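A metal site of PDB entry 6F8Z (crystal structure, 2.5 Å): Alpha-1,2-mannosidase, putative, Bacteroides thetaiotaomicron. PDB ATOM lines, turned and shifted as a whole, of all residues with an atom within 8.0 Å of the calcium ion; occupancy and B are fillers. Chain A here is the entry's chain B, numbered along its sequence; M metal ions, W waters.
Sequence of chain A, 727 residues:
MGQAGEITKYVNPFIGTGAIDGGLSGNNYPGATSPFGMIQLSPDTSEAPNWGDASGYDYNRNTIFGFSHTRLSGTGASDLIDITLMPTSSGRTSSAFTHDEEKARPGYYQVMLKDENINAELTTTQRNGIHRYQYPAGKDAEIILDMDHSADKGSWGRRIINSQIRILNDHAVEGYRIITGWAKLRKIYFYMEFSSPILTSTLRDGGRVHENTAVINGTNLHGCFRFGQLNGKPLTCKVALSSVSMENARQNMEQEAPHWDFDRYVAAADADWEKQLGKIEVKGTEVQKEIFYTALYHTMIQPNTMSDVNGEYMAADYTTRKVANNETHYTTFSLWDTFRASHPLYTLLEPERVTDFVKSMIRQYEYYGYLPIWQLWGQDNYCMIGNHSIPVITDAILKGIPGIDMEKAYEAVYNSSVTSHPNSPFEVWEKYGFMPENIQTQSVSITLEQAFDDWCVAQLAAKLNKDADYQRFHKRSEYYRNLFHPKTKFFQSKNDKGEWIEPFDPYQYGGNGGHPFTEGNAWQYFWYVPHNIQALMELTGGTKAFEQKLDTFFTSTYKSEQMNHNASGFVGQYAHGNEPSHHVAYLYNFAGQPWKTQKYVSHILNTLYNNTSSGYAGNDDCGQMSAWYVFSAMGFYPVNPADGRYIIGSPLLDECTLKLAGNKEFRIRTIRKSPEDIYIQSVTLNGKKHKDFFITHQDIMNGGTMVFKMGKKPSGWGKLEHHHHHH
The backbone NH of Gly 577 sits close to the backbone carbonyl oxygen of Ala 617. The backbone NH of Asp 621 lies within hydrogen-bond range of the backbone carbonyl oxygen of Gly 74 (2.9 Å).
The calcium ion is bound by the side-chain carboxylate (OE2) of Glu 579 (2.3 Å), water W5 (2.3 Å), water W2 (2.3 Å), water W4 (2.3 Å), water W3 (2.3 Å), water W1 (2.3 Å), the side-chain carboxylate (OD2) of Asp 621 (2.4 Å) and the backbone carbonyl oxygen (O) of Gly 577 (2.4 Å). The calcium ion has eight donor atoms within binding distance.
Water W4 lies within hydrogen-bond range of the backbone carbonyl oxygen (O) of Asn 619 and the side-chain sulfur (SD) of Met 625. Water W3 bridges the side-chain carboxylate (OD1) of Asp 337 and the side-chain carboxylate (OD1) of Asp 621.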
ATOM      1  N   GLY A  74       4.257 -16.901 -20.465  1.00  0.00           N
ATOM      2  CA  GLY A  74       5.191 -17.294 -21.507  1.00  0.00           C
ATOM      3  C   GLY A  74       5.297 -18.770 -21.802  1.00  0.00           C
ATOM      4  O   GLY A  74       6.285 -19.195 -22.378  1.00  0.00           O
ATOM      5  N   TRP A 336      13.188 -26.973 -17.708  1.00  0.00           N
ATOM      6  CA  TRP A 336      13.967 -27.097 -18.947  1.00  0.00           C
ATOM      7  C   TRP A 336      14.444 -25.741 -19.481  1.00  0.00           C
ATOM      8  O   TRP A 336      15.577 -25.636 -19.973  1.00  0.00           O
ATOM      9  CB  TRP A 336      13.167 -27.845 -20.031  1.00  0.00           C
ATOM     10  CG  TRP A 336      13.942 -28.166 -21.276  1.00  0.00           C
ATOM     11  CD1 TRP A 336      14.852 -29.171 -21.452  1.00  0.00           C
ATOM     12  CD2 TRP A 336      13.858 -27.492 -22.510  1.00  0.00           C
ATOM     13  NE1 TRP A 336      15.336 -29.150 -22.732  1.00  0.00           N
ATOM     14  CE2 TRP A 336      14.739 -28.124 -23.406  1.00  0.00           C
ATOM     15  CE3 TRP A 336      13.114 -26.395 -22.959  1.00  0.00           C
ATOM     16  CZ2 TRP A 336      14.897 -27.696 -24.734  1.00  0.00           C
ATOM     17  CZ3 TRP A 336      13.273 -25.967 -24.287  1.00  0.00           C
ATOM     18  CH2 TRP A 336      14.155 -26.625 -25.151  1.00  0.00           C
ATOM     19  N   ASP A 337      13.602 -24.712 -19.346  1.00  0.00           N
ATOM     20  CA  ASP A 337      14.006 -23.334 -19.641  1.00  0.00           C
ATOM     21  C   ASP A 337      14.785 -22.691 -18.485  1.00  0.00           C
ATOM     22  O   ASP A 337      15.893 -22.201 -18.688  1.00  0.00           O
ATOM     23  CB  ASP A 337      12.813 -22.462 -19.972  1.00  0.00           C
ATOM     24  CG  ASP A 337      11.892 -23.108 -20.985  1.00  0.00           C
ATOM     25  OD1 ASP A 337      12.314 -23.303 -22.144  1.00  0.00           O
ATOM     26  OD2 ASP A 337      10.723 -23.394 -20.625  1.00  0.00           O
ATOM     27  N   MET A 384       9.092 -31.437 -21.708  1.00  0.00           N
ATOM     28  CA  MET A 384      10.484 -31.347 -22.183  1.00  0.00           C
ATOM     29  C   MET A 384      11.326 -32.522 -21.667  1.00  0.00           C
ATOM     30  O   MET A 384      10.814 -33.628 -21.612  1.00  0.00           O
ATOM     31  CB  MET A 384      11.104 -29.963 -21.880  1.00  0.00           C
ATOM     32  CG  MET A 384      10.248 -28.769 -22.264  1.00  0.00           C
ATOM     33  SD  MET A 384       9.547 -28.837 -23.928  1.00  0.00           S
ATOM     34  CE  MET A 384      11.024 -28.955 -24.925  1.00  0.00           C
ATOM     35  N   GLU A 519      12.978 -30.044 -29.949  1.00  0.00           N
ATOM     36  CA  GLU A 519      12.916 -28.721 -30.603  1.00  0.00           C
ATOM     37  C   GLU A 519      14.302 -28.145 -30.983  1.00  0.00           C
ATOM     38  O   GLU A 519      14.938 -27.468 -30.185  1.00  0.00           O
ATOM     39  CB  GLU A 519      12.153 -27.721 -29.723  1.00  0.00           C
ATOM     40  CG  GLU A 519      10.638 -27.922 -29.754  1.00  0.00           C
ATOM     41  CD  GLU A 519       9.935 -27.524 -28.457  1.00  0.00           C
ATOM     42  OE1 GLU A 519      10.428 -26.621 -27.747  1.00  0.00           O
ATOM     43  OE2 GLU A 519       8.876 -28.128 -28.149  1.00  0.00           O
ATOM     44  N   ALA A 575      18.833 -19.494 -33.305  1.00  0.00           N
ATOM     45  CA  ALA A 575      17.502 -18.965 -33.018  1.00  0.00           C
ATOM     46  C   ALA A 575      17.477 -18.558 -31.556  1.00  0.00           C
ATOM     47  O   ALA A 575      17.612 -19.412 -30.682  1.00  0.00           O
ATOM     48  CB  ALA A 575      16.441 -20.024 -33.285  1.00  0.00           C
ATOM     49  N   HIS A 576      17.316 -17.266 -31.279  1.00  0.00           N
ATOM     50  CA  HIS A 576      17.333 -16.821 -29.891  1.00  0.00           C
ATOM     51  C   HIS A 576      16.209 -17.401 -29.022  1.00  0.00           C
ATOM     52  O   HIS A 576      16.409 -17.554 -27.810  1.00  0.00           O
ATOM     53  CB  HIS A 576      17.370 -15.305 -29.763  1.00  0.00           C
ATOM     54  CG  HIS A 576      17.737 -14.856 -28.379  1.00  0.00           C
ATOM     55  ND1 HIS A 576      18.893 -15.280 -27.765  1.00  0.00           N
ATOM     56  CD2 HIS A 576      17.071 -14.114 -27.471  1.00  0.00           C
ATOM     57  CE1 HIS A 576      18.945 -14.774 -26.548  1.00  0.00           C
ATOM     58  NE2 HIS A 576      17.851 -14.069 -26.339  1.00  0.00           N
ATOM     59  N   GLY A 577      15.084 -17.782 -29.639  1.00  0.00           N
ATOM     60  CA  GLY A 577      13.980 -18.484 -28.936  1.00  0.00           C
ATOM     61  C   GLY A 577      14.283 -19.879 -28.373  1.00  0.00           C
ATOM     62  O   GLY A 577      13.542 -20.387 -27.499  1.00  0.00           O
ATOM     63  N   ASN A 578      15.367 -20.493 -28.869  1.00  0.00           N
ATOM     64  CA  ASN A 578      15.778 -21.852 -28.481  1.00  0.00           C
ATOM     65  C   ASN A 578      16.711 -21.905 -27.286  1.00  0.00           C
ATOM     66  O   ASN A 578      17.921 -21.704 -27.458  1.00  0.00           O
ATOM     67  CB  ASN A 578      16.537 -22.551 -29.648  1.00  0.00           C
ATOM     68  CG  ASN A 578      15.606 -23.092 -30.731  1.00  0.00           C
ATOM     69  OD1 ASN A 578      14.470 -22.634 -30.906  1.00  0.00           O
ATOM     70  ND2 ASN A 578      16.103 -24.092 -31.466  1.00  0.00           N
ATOM     71  N   GLU A 579      16.203 -22.249 -26.113  1.00  0.00           N
ATOM     72  CA  GLU A 579      17.057 -22.204 -24.911  1.00  0.00           C
ATOM     73  C   GLU A 579      18.337 -23.058 -24.992  1.00  0.00           C
ATOM     74  O   GLU A 579      19.345 -22.694 -24.362  1.00  0.00           O
ATOM     75  CB  GLU A 579      16.366 -22.527 -23.577  1.00  0.00           C
ATOM     76  CG  GLU A 579      14.860 -22.576 -23.502  1.00  0.00           C
ATOM     77  CD  GLU A 579      14.169 -21.251 -23.627  1.00  0.00           C
ATOM     78  OE1 GLU A 579      14.087 -20.503 -22.661  1.00  0.00           O
ATOM     79  OE2 GLU A 579      13.630 -20.997 -24.693  1.00  0.00           O
ATOM     80  N   PRO A 580      18.313 -24.185 -25.745  1.00  0.00           N
ATOM     81  CA  PRO A 580      19.556 -24.973 -25.781  1.00  0.00           C
ATOM     82  C   PRO A 580      20.773 -24.245 -26.345  1.00  0.00           C
ATOM     83  O   PRO A 580      21.895 -24.592 -25.991  1.00  0.00           O
ATOM     84  CB  PRO A 580      19.172 -26.181 -26.640  1.00  0.00           C
ATOM     85  CG  PRO A 580      17.724 -26.359 -26.326  1.00  0.00           C
ATOM     86  CD  PRO A 580      17.192 -24.952 -26.329  1.00  0.00           C
ATOM     87  N   HIS A 582      21.203 -20.815 -25.848  1.00  0.00           N
ATOM     88  CA  HIS A 582      21.236 -19.499 -25.162  1.00  0.00           C
ATOM     89  C   HIS A 582      22.626 -19.097 -24.681  1.00  0.00           C
ATOM     90  O   HIS A 582      22.942 -17.921 -24.575  1.00  0.00           O
ATOM     91  CB  HIS A 582      20.269 -19.468 -23.976  1.00  0.00           C
ATOM     92  CG  HIS A 582      18.902 -18.955 -24.297  1.00  0.00           C
ATOM     93  ND1 HIS A 582      17.966 -18.717 -23.326  1.00  0.00           N
ATOM     94  CD2 HIS A 582      18.335 -18.567 -25.466  1.00  0.00           C
ATOM     95  CE1 HIS A 582      16.866 -18.234 -23.883  1.00  0.00           C
ATOM     96  NE2 HIS A 582      17.065 -18.131 -25.184  1.00  0.00           N
ATOM     97  N   ALA A 617      11.943 -12.820 -28.870  1.00  0.00           N
ATOM     98  CA  ALA A 617      12.134 -13.702 -30.027  1.00  0.00           C
ATOM     99  C   ALA A 617      11.562 -15.108 -29.805  1.00  0.00           C
ATOM    100  O   ALA A 617      12.207 -16.109 -30.098  1.00  0.00           O
ATOM    101  CB  ALA A 617      13.623 -13.791 -30.342  1.00  0.00           C
ATOM    102  N   GLY A 618      10.322 -15.177 -29.336  1.00  0.00           N
ATOM    103  CA  GLY A 618       9.709 -16.435 -28.893  1.00  0.00           C
ATOM    104  C   GLY A 618       9.059 -16.264 -27.535  1.00  0.00           C
ATOM    105  O   GLY A 618       9.142 -15.191 -26.919  1.00  0.00           O
ATOM    106  N   ASN A 619       8.392 -17.318 -27.064  1.00  0.00           N
ATOM    107  CA  ASN A 619       7.711 -17.270 -25.772  1.00  0.00           C
ATOM    108  C   ASN A 619       8.689 -16.978 -24.645  1.00  0.00           C
ATOM    109  O   ASN A 619       9.804 -17.497 -24.643  1.00  0.00           O
ATOM    110  CB  ASN A 619       7.021 -18.588 -25.437  1.00  0.00           C
ATOM    111  CG  ASN A 619       5.903 -18.984 -26.399  1.00  0.00           C
ATOM    112  OD1 ASN A 619       5.523 -20.144 -26.424  1.00  0.00           O
ATOM    113  ND2 ASN A 619       5.328 -18.028 -27.133  1.00  0.00           N
ATOM    114  N   ASP A 620       8.255 -16.195 -23.656  1.00  0.00           N
ATOM    115  CA  ASP A 620       9.126 -15.792 -22.540  1.00  0.00           C
ATOM    116  C   ASP A 620       9.670 -16.985 -21.696  1.00  0.00           C
ATOM    117  O   ASP A 620      10.755 -16.879 -21.101  1.00  0.00           O
ATOM    118  CB  ASP A 620       8.405 -14.763 -21.664  1.00  0.00           C
ATOM    119  CG  ASP A 620       9.348 -13.951 -20.765  1.00  0.00           C
ATOM    120  OD1 ASP A 620      10.553 -13.801 -21.058  1.00  0.00           O
ATOM    121  OD2 ASP A 620       8.845 -13.453 -19.742  1.00  0.00           O
ATOM    122  N   ASP A 621       8.921 -18.089 -21.659  1.00  0.00           N
ATOM    123  CA  ASP A 621       9.330 -19.345 -20.992  1.00  0.00           C
ATOM    124  C   ASP A 621       9.487 -19.163 -19.492  1.00  0.00           C
ATOM    125  O   ASP A 621      10.510 -19.518 -18.910  1.00  0.00           O
ATOM    126  CB  ASP A 621      10.611 -19.955 -21.640  1.00  0.00           C
ATOM    127  CG  ASP A 621      10.454 -20.268 -23.136  1.00  0.00           C
ATOM    128  OD1 ASP A 621       9.316 -20.506 -23.569  1.00  0.00           O
ATOM    129  OD2 ASP A 621      11.470 -20.294 -23.901  1.00  0.00           O
ATOM    130  N   GLN A 624      12.614 -16.911 -18.708  1.00  0.00           N
ATOM    131  CA  GLN A 624      13.985 -17.262 -19.143  1.00  0.00           C
ATOM    132  C   GLN A 624      14.507 -16.361 -20.268  1.00  0.00           C
ATOM    133  O   GLN A 624      15.687 -16.010 -20.284  1.00  0.00           O
ATOM    134  CB  GLN A 624      14.092 -18.749 -19.518  1.00  0.00           C
ATOM    135  CG  GLN A 624      15.391 -19.199 -20.151  1.00  0.00           C
ATOM    136  CD  GLN A 624      16.624 -19.016 -19.283  1.00  0.00           C
ATOM    137  OE1 GLN A 624      16.574 -19.046 -18.052  1.00  0.00           O
ATOM    138  NE2 GLN A 624      17.764 -18.852 -19.945  1.00  0.00           N
ATOM    139  N   MET A 625      13.642 -15.978 -21.205  1.00  0.00           N
ATOM    140  CA  MET A 625      14.045 -15.039 -22.259  1.00  0.00           C
ATOM    141  C   MET A 625      14.367 -13.692 -21.637  1.00  0.00           C
ATOM    142  O   MET A 625      15.335 -13.028 -22.015  1.00  0.00           O
ATOM    143  CB  MET A 625      12.940 -14.881 -23.310  1.00  0.00           C
ATOM    144  CG  MET A 625      12.662 -16.125 -24.147  1.00  0.00           C
ATOM    145  SD  MET A 625      13.960 -16.609 -25.320  1.00  0.00           S
ATOM    146  CE  MET A 625      13.802 -15.292 -26.530  1.00  0.00           C
HETATM  147 CA    CA M   1      11.799 -21.139 -26.082  1.00  0.00          CA
HETATM  148  O   HOH W   1      11.185 -21.395 -28.330  1.00  0.00           O
HETATM  149  O   HOH W   2      12.615 -23.149 -26.922  1.00  0.00           O
HETATM  150  O   HOH W   3      11.094 -22.855 -24.666  1.00  0.00           O
HETATM  151  O   HOH W   4      11.500 -18.861 -26.461  1.00  0.00           O
HETATM  152  O   HOH W   5       9.497 -21.317 -26.351  1.00  0.00           O
